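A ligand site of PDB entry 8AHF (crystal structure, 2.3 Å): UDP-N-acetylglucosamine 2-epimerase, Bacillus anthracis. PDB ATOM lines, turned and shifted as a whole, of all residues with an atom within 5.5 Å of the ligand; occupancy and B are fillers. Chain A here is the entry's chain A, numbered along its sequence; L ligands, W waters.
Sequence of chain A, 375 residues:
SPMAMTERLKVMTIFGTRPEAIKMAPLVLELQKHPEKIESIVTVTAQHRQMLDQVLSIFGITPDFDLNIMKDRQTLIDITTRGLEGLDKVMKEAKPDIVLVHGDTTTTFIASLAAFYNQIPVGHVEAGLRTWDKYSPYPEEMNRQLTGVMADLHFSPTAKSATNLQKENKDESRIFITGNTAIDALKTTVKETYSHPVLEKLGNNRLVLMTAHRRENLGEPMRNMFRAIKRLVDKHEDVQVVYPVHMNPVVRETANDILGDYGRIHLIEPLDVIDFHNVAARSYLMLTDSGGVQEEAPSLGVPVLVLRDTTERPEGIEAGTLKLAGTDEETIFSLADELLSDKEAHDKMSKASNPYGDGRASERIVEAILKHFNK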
ATOM      1  N   LYS A  23     -26.243  39.475 -16.225  1.00  0.00           N
ATOM      2  CA  LYS A  23     -27.438  40.284 -16.460  1.00  0.00           C
ATOM      3  C   LYS A  23     -27.091  41.705 -16.937  1.00  0.00           C
ATOM      4  O   LYS A  23     -27.955  42.338 -17.575  1.00  0.00           O
ATOM      5  CB  LYS A  23     -28.335  40.317 -15.207  1.00  0.00           C
ATOM      6  CG  LYS A  23     -28.788  38.942 -14.728  1.00  0.00           C
ATOM      7  CD  LYS A  23     -29.194  38.847 -13.275  1.00  0.00           C
ATOM      8  CE  LYS A  23     -29.298  37.401 -12.785  1.00  0.00           C
ATOM      9  NZ  LYS A  23     -29.889  37.278 -11.417  1.00  0.00           N
ATOM     10  N   LEU A 186     -27.065  35.225 -23.903  1.00  0.00           N
ATOM     11  CA  LEU A 186     -26.926  33.928 -24.538  1.00  0.00           C
ATOM     12  C   LEU A 186     -26.361  34.042 -25.957  1.00  0.00           C
ATOM     13  O   LEU A 186     -25.606  33.150 -26.359  1.00  0.00           O
ATOM     14  CB  LEU A 186     -28.274  33.217 -24.581  1.00  0.00           C
ATOM     15  CG  LEU A 186     -28.983  33.046 -23.256  1.00  0.00           C
ATOM     16  CD1 LEU A 186     -30.404  32.535 -23.512  1.00  0.00           C
ATOM     17  CD2 LEU A 186     -28.198  32.134 -22.337  1.00  0.00           C
ATOM     18  N   THR A 211     -31.747  20.788 -12.235  1.00  0.00           N
ATOM     19  CA  THR A 211     -31.294  21.688 -11.185  1.00  0.00           C
ATOM     20  C   THR A 211     -32.360  21.706 -10.080  1.00  0.00           C
ATOM     21  O   THR A 211     -33.535  21.672 -10.359  1.00  0.00           O
ATOM     22  CB  THR A 211     -31.009  23.100 -11.722  1.00  0.00           C
ATOM     23  OG1 THR A 211     -32.221  23.683 -12.197  1.00  0.00           O
ATOM     24  CG2 THR A 211     -30.016  23.075 -12.860  1.00  0.00           C
ATOM     25  N   ALA A 212     -31.916  21.729  -8.835  1.00  0.00           N
ATOM     26  CA  ALA A 212     -32.802  21.749  -7.685  1.00  0.00           C
ATOM     27  C   ALA A 212     -32.051  22.405  -6.525  1.00  0.00           C
ATOM     28  O   ALA A 212     -30.905  22.033  -6.268  1.00  0.00           O
ATOM     29  CB  ALA A 212     -33.247  20.340  -7.356  1.00  0.00           C
ATOM     30  N   HIS A 213     -32.677  23.405  -5.891  1.00  0.00           N
ATOM     31  CA  HIS A 213     -32.197  23.948  -4.637  1.00  0.00           C
ATOM     32  C   HIS A 213     -32.276  22.843  -3.590  1.00  0.00           C
ATOM     33  O   HIS A 213     -33.226  22.074  -3.607  1.00  0.00           O
ATOM     34  CB  HIS A 213     -33.030  25.166  -4.218  1.00  0.00           C
ATOM     35  CG  HIS A 213     -33.030  26.300  -5.195  1.00  0.00           C
ATOM     36  ND1 HIS A 213     -31.884  26.905  -5.669  1.00  0.00           N
ATOM     37  CD2 HIS A 213     -34.089  26.970  -5.723  1.00  0.00           C
ATOM     38  CE1 HIS A 213     -32.226  27.897  -6.481  1.00  0.00           C
ATOM     39  NE2 HIS A 213     -33.591  27.957  -6.512  1.00  0.00           N
ATOM     40  N   PRO A 244     -26.041  18.884 -11.630  1.00  0.00           N
ATOM     41  CA  PRO A 244     -24.926  19.636 -11.027  1.00  0.00           C
ATOM     42  C   PRO A 244     -25.380  20.167  -9.660  1.00  0.00           C
ATOM     43  O   PRO A 244     -26.409  20.856  -9.605  1.00  0.00           O
ATOM     44  CB  PRO A 244     -24.624  20.753 -12.050  1.00  0.00           C
ATOM     45  CG  PRO A 244     -25.500  20.432 -13.231  1.00  0.00           C
ATOM     46  CD  PRO A 244     -26.696  19.677 -12.668  1.00  0.00           C
ATOM     47  N   VAL A 245     -24.702  19.764  -8.587  1.00  0.00           N
ATOM     48  CA  VAL A 245     -25.101  19.972  -7.185  1.00  0.00           C
ATOM     49  C   VAL A 245     -23.879  19.820  -6.260  1.00  0.00           C
ATOM     50  O   VAL A 245     -23.021  18.960  -6.547  1.00  0.00           O
ATOM     51  CB  VAL A 245     -26.190  18.976  -6.742  1.00  0.00           C
ATOM     52  CG1 VAL A 245     -25.734  17.520  -6.889  1.00  0.00           C
ATOM     53  CG2 VAL A 245     -26.671  19.238  -5.313  1.00  0.00           C
ATOM     54  N   GLU A 269     -20.259  18.465  -9.836  1.00  0.00           N
ATOM     55  CA  GLU A 269     -20.100  19.737  -9.123  1.00  0.00           C
ATOM     56  C   GLU A 269     -20.822  20.825  -9.916  1.00  0.00           C
ATOM     57  O   GLU A 269     -20.909  20.744 -11.131  1.00  0.00           O
ATOM     58  CB  GLU A 269     -18.607  20.042  -8.903  1.00  0.00           C
ATOM     59  CG  GLU A 269     -17.962  19.269  -7.747  1.00  0.00           C
ATOM     60  CD  GLU A 269     -18.628  19.447  -6.390  1.00  0.00           C
ATOM     61  OE1 GLU A 269     -19.045  18.410  -5.802  1.00  0.00           O
ATOM     62  OE2 GLU A 269     -18.766  20.630  -5.895  1.00  0.00           O
ATOM     63  N   PRO A 270     -21.359  21.867  -9.252  1.00  0.00           N
ATOM     64  CA  PRO A 270     -22.025  22.961  -9.965  1.00  0.00           C
ATOM     65  C   PRO A 270     -21.236  23.459 -11.168  1.00  0.00           C
ATOM     66  O   PRO A 270     -20.030  23.444 -11.168  1.00  0.00           O
ATOM     67  CB  PRO A 270     -22.083  24.037  -8.861  1.00  0.00           C
ATOM     68  CG  PRO A 270     -22.383  23.213  -7.626  1.00  0.00           C
ATOM     69  CD  PRO A 270     -21.455  22.031  -7.784  1.00  0.00           C
ATOM     70  N   LEU A 271     -21.925  23.893 -12.210  1.00  0.00           N
ATOM     71  CA  LEU A 271     -21.321  24.433 -13.408  1.00  0.00           C
ATOM     72  C   LEU A 271     -21.267  25.953 -13.286  1.00  0.00           C
ATOM     73  O   LEU A 271     -22.239  26.521 -12.805  1.00  0.00           O
ATOM     74  CB  LEU A 271     -22.211  24.031 -14.590  1.00  0.00           C
ATOM     75  CG  LEU A 271     -22.210  22.544 -14.907  1.00  0.00           C
ATOM     76  CD1 LEU A 271     -23.161  22.254 -16.063  1.00  0.00           C
ATOM     77  CD2 LEU A 271     -20.804  22.105 -15.227  1.00  0.00           C
ATOM     78  N   ASP A 272     -20.171  26.560 -13.744  1.00  0.00           N
ATOM     79  CA  ASP A 272     -20.058  28.006 -13.824  1.00  0.00           C
ATOM     80  C   ASP A 272     -20.984  28.440 -14.976  1.00  0.00           C
ATOM     81  O   ASP A 272     -21.325  27.607 -15.807  1.00  0.00           O
ATOM     82  CB  ASP A 272     -18.576  28.411 -13.907  1.00  0.00           C
ATOM     83  CG  ASP A 272     -17.807  28.178 -15.212  1.00  0.00           C
ATOM     84  OD1 ASP A 272     -18.416  28.139 -16.314  1.00  0.00           O
ATOM     85  OD2 ASP A 272     -16.565  28.037 -15.115  1.00  0.00           O
ATOM     86  N   VAL A 273     -21.313  29.745 -15.048  1.00  0.00           N
ATOM     87  CA  VAL A 273     -22.486  30.188 -15.776  1.00  0.00           C
ATOM     88  C   VAL A 273     -22.300  29.896 -17.247  1.00  0.00           C
ATOM     89  O   VAL A 273     -23.240  29.528 -17.946  1.00  0.00           O
ATOM     90  CB  VAL A 273     -22.843  31.677 -15.476  1.00  0.00           C
ATOM     91  CG1 VAL A 273     -21.711  32.655 -15.758  1.00  0.00           C
ATOM     92  CG2 VAL A 273     -24.116  32.102 -16.219  1.00  0.00           C
ATOM     93  N   PHE A 276     -22.739  26.237 -17.864  1.00  0.00           N
ATOM     94  CA  PHE A 276     -24.169  25.942 -17.695  1.00  0.00           C
ATOM     95  C   PHE A 276     -24.936  26.285 -18.961  1.00  0.00           C
ATOM     96  O   PHE A 276     -25.621  25.452 -19.507  1.00  0.00           O
ATOM     97  CB  PHE A 276     -24.785  26.640 -16.494  1.00  0.00           C
ATOM     98  CG  PHE A 276     -26.183  26.159 -16.170  1.00  0.00           C
ATOM     99  CD1 PHE A 276     -26.397  24.992 -15.431  1.00  0.00           C
ATOM    100  CD2 PHE A 276     -27.280  26.834 -16.647  1.00  0.00           C
ATOM    101  CE1 PHE A 276     -27.707  24.547 -15.164  1.00  0.00           C
ATOM    102  CE2 PHE A 276     -28.576  26.405 -16.381  1.00  0.00           C
ATOM    103  CZ  PHE A 276     -28.780  25.276 -15.609  1.00  0.00           C
ATOM    104  N   HIS A 277     -24.756  27.516 -19.447  1.00  0.00           N
ATOM    105  CA  HIS A 277     -25.334  27.993 -20.683  1.00  0.00           C
ATOM    106  C   HIS A 277     -25.050  27.001 -21.813  1.00  0.00           C
ATOM    107  O   HIS A 277     -25.901  26.745 -22.651  1.00  0.00           O
ATOM    108  CB  HIS A 277     -24.768  29.401 -21.010  1.00  0.00           C
ATOM    109  CG  HIS A 277     -25.323  30.561 -20.238  1.00  0.00           C
ATOM    110  ND1 HIS A 277     -25.088  31.876 -20.595  1.00  0.00           N
ATOM    111  CD2 HIS A 277     -26.118  30.584 -19.117  1.00  0.00           C
ATOM    112  CE1 HIS A 277     -25.731  32.678 -19.728  1.00  0.00           C
ATOM    113  NE2 HIS A 277     -26.399  31.882 -18.798  1.00  0.00           N
ATOM    114  N   ALA A 280     -26.777  23.556 -21.130  1.00  0.00           N
ATOM    115  CA  ALA A 280     -28.227  23.737 -21.256  1.00  0.00           C
ATOM    116  C   ALA A 280     -28.618  23.883 -22.731  1.00  0.00           C
ATOM    117  O   ALA A 280     -29.623  23.315 -23.172  1.00  0.00           O
ATOM    118  CB  ALA A 280     -28.696  24.925 -20.485  1.00  0.00           C
ATOM    119  N   SER A 290     -35.415  26.576 -10.549  1.00  0.00           N
ATOM    120  CA  SER A 290     -34.789  27.888 -10.669  1.00  0.00           C
ATOM    121  C   SER A 290     -35.670  28.844 -11.472  1.00  0.00           C
ATOM    122  O   SER A 290     -36.168  28.521 -12.556  1.00  0.00           O
ATOM    123  CB  SER A 290     -33.386  27.784 -11.243  1.00  0.00           C
ATOM    124  OG  SER A 290     -32.944  29.036 -11.820  1.00  0.00           O
ATOM    125  N   GLY A 291     -35.884  30.053 -10.944  1.00  0.00           N
ATOM    126  CA  GLY A 291     -36.614  31.083 -11.667  1.00  0.00           C
ATOM    127  C   GLY A 291     -35.830  31.498 -12.896  1.00  0.00           C
ATOM    128  O   GLY A 291     -36.431  31.642 -13.946  1.00  0.00           O
ATOM    129  N   GLY A 292     -34.495  31.637 -12.754  1.00  0.00           N
ATOM    130  CA  GLY A 292     -33.626  32.062 -13.844  1.00  0.00           C
ATOM    131  C   GLY A 292     -33.657  31.058 -15.002  1.00  0.00           C
ATOM    132  O   GLY A 292     -33.776  31.467 -16.175  1.00  0.00           O
ATOM    133  N   VAL A 293     -33.596  29.751 -14.664  1.00  0.00           N
ATOM    134  CA  VAL A 293     -33.672  28.717 -15.685  1.00  0.00           C
ATOM    135  C   VAL A 293     -35.013  28.819 -16.419  1.00  0.00           C
ATOM    136  O   VAL A 293     -35.054  28.718 -17.674  1.00  0.00           O
ATOM    137  CB  VAL A 293     -33.402  27.308 -15.132  1.00  0.00           C
ATOM    138  CG1 VAL A 293     -33.658  26.227 -16.179  1.00  0.00           C
ATOM    139  CG2 VAL A 293     -32.007  27.151 -14.588  1.00  0.00           C
ATOM    140  N   GLN A 294     -36.108  29.055 -15.672  1.00  0.00           N
ATOM    141  CA  GLN A 294     -37.455  29.193 -16.232  1.00  0.00           C
ATOM    142  C   GLN A 294     -37.568  30.356 -17.217  1.00  0.00           C
ATOM    143  O   GLN A 294     -38.292  30.253 -18.242  1.00  0.00           O
ATOM    144  CB  GLN A 294     -38.492  29.344 -15.131  1.00  0.00           C
ATOM    145  CG  GLN A 294     -38.770  28.046 -14.373  1.00  0.00           C
ATOM    146  CD  GLN A 294     -39.790  28.232 -13.252  1.00  0.00           C
ATOM    147  OE1 GLN A 294     -40.993  28.393 -13.480  1.00  0.00           O
ATOM    148  NE2 GLN A 294     -39.312  28.219 -12.020  1.00  0.00           N
ATOM    149  N   GLU A 296     -34.727  31.852 -18.727  1.00  0.00           N
ATOM    150  CA  GLU A 296     -33.612  31.885 -19.688  1.00  0.00           C
ATOM    151  C   GLU A 296     -33.597  30.660 -20.621  1.00  0.00           C
ATOM    152  O   GLU A 296     -33.660  30.839 -21.844  1.00  0.00           O
ATOM    153  CB  GLU A 296     -32.267  32.088 -18.967  1.00  0.00           C
ATOM    154  CG  GLU A 296     -32.177  33.420 -18.236  1.00  0.00           C
ATOM    155  CD  GLU A 296     -31.207  33.496 -17.071  1.00  0.00           C
ATOM    156  OE1 GLU A 296     -30.129  32.817 -17.135  1.00  0.00           O
ATOM    157  OE2 GLU A 296     -31.496  34.279 -16.114  1.00  0.00           O
ATOM    158  N   ALA A 297     -33.608  29.432 -20.064  1.00  0.00           N
ATOM    159  CA  ALA A 297     -33.392  28.169 -20.791  1.00  0.00           C
ATOM    160  C   ALA A 297     -34.310  28.036 -22.006  1.00  0.00           C
ATOM    161  O   ALA A 297     -33.919  27.484 -23.041  1.00  0.00           O
ATOM    162  CB  ALA A 297     -33.532  26.981 -19.859  1.00  0.00           C
ATOM    163  N   LEU A 300     -33.109  28.950 -25.440  1.00  0.00           N
ATOM    164  CA  LEU A 300     -32.202  27.975 -26.023  1.00  0.00           C
ATOM    165  C   LEU A 300     -32.953  26.831 -26.717  1.00  0.00           C
ATOM    166  O   LEU A 300     -32.341  25.929 -27.279  1.00  0.00           O
ATOM    167  CB  LEU A 300     -31.307  27.424 -24.893  1.00  0.00           C
ATOM    168  CG  LEU A 300     -30.323  28.416 -24.274  1.00  0.00           C
ATOM    169  CD1 LEU A 300     -29.666  27.859 -23.011  1.00  0.00           C
ATOM    170  CD2 LEU A 300     -29.260  28.813 -25.326  1.00  0.00           C
HETATM  171  N1  LIG L   1     -30.959  31.816 -11.496  1.00  0.00           N
HETATM  172  N2  LIG L   1     -28.255  24.985 -10.902  1.00  0.00           N
HETATM  173  C1  LIG L   1     -29.401  31.150 -14.488  1.00  0.00           C
HETATM  174  C2  LIG L   1     -28.844  29.998 -15.315  1.00  0.00           C
HETATM  175  C3  LIG L   1     -30.097  29.581 -17.298  1.00  0.00           C
HETATM  176  C4  LIG L   1     -28.194  29.126 -14.242  1.00  0.00           C
HETATM  177  C5  LIG L   1     -29.341  28.405 -12.079  1.00  0.00           C
HETATM  178  C6  LIG L   1     -28.932  26.110 -11.184  1.00  0.00           C
HETATM  179  C7  LIG L   1     -26.329  26.076 -11.940  1.00  0.00           C
HETATM  180  C8  LIG L   1     -31.316  33.231 -11.417  1.00  0.00           C
HETATM  181  C9  LIG L   1     -29.803  31.395 -11.996  1.00  0.00           C
HETATM  182  O1  LIG L   1     -28.708  31.754 -11.561  1.00  0.00           O
HETATM  183  C10 LIG L   1     -29.944  30.476 -13.213  1.00  0.00           C
HETATM  184  O2  LIG L   1     -29.923  29.273 -15.927  1.00  0.00           O
HETATM  185  F1  LIG L   1     -31.205  29.016 -17.787  1.00  0.00           F
HETATM  186  F2  LIG L   1     -29.071  29.044 -17.976  1.00  0.00           F
HETATM  187  N3  LIG L   1     -29.121  29.256 -13.105  1.00  0.00           N
HETATM  188  O3  LIG L   1     -30.310  28.552 -11.338  1.00  0.00           O
HETATM  189  C11 LIG L   1     -28.406  27.251 -11.846  1.00  0.00           C
HETATM  190  C12 LIG L   1     -26.954  24.977 -11.280  1.00  0.00           C
HETATM  191  C13 LIG L   1     -26.002  24.025 -11.124  1.00  0.00           C
HETATM  192  N4  LIG L   1     -24.883  24.467 -11.708  1.00  0.00           N
HETATM  193  N5  LIG L   1     -25.042  25.748 -12.183  1.00  0.00           N
HETATM  194  C14 LIG L   1     -27.071  27.241 -12.240  1.00  0.00           C
HETATM  195  O   HOH W   1     -25.821  30.454 -11.220  1.00  0.00           O
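The backbone NH of Val 293 lies within hydrogen-bond range of the side-chain hydroxyl of Ser 290, at 3.0 Å.
N of Gly 292 lies within hydrogen-bond range of OG of Ser 290 (3.2 Å).
The backbone carbonyl oxygen (O) of Ser 290 is in hydrogen-bond range of the side-chain amide nitrogen (NE2) of Gln 294 (3.2 Å).
A nitrogen (N4) of the ligand lies close to the backbone NH (N) of Leu 271, at 3.1 Å.
The backbone carbonyl oxygen of Leu 271 lies close to a nitrogen (N5) of the ligand, at 3.0 Å.
OG of Ser 290 lies within hydrogen-bond range of O3 of the ligand, at 2.7 Å.
The backbone NH of Ala 297 lies close to a fluorine (F1) of the ligand (3.3 Å).
Merely in contact with the ligand: Phe 276, Glu 296, Thr 211, Val 293, His 277, Pro 244, Gly 292 and Pro 270.
Hydrophobic or aromatic side chains that line the ligand: Pro 244, Leu 271, Phe 276, His 277, Val 293 and Ala 297.
Of the 23 residues printed, 11 come within 4 Å of the ligand.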
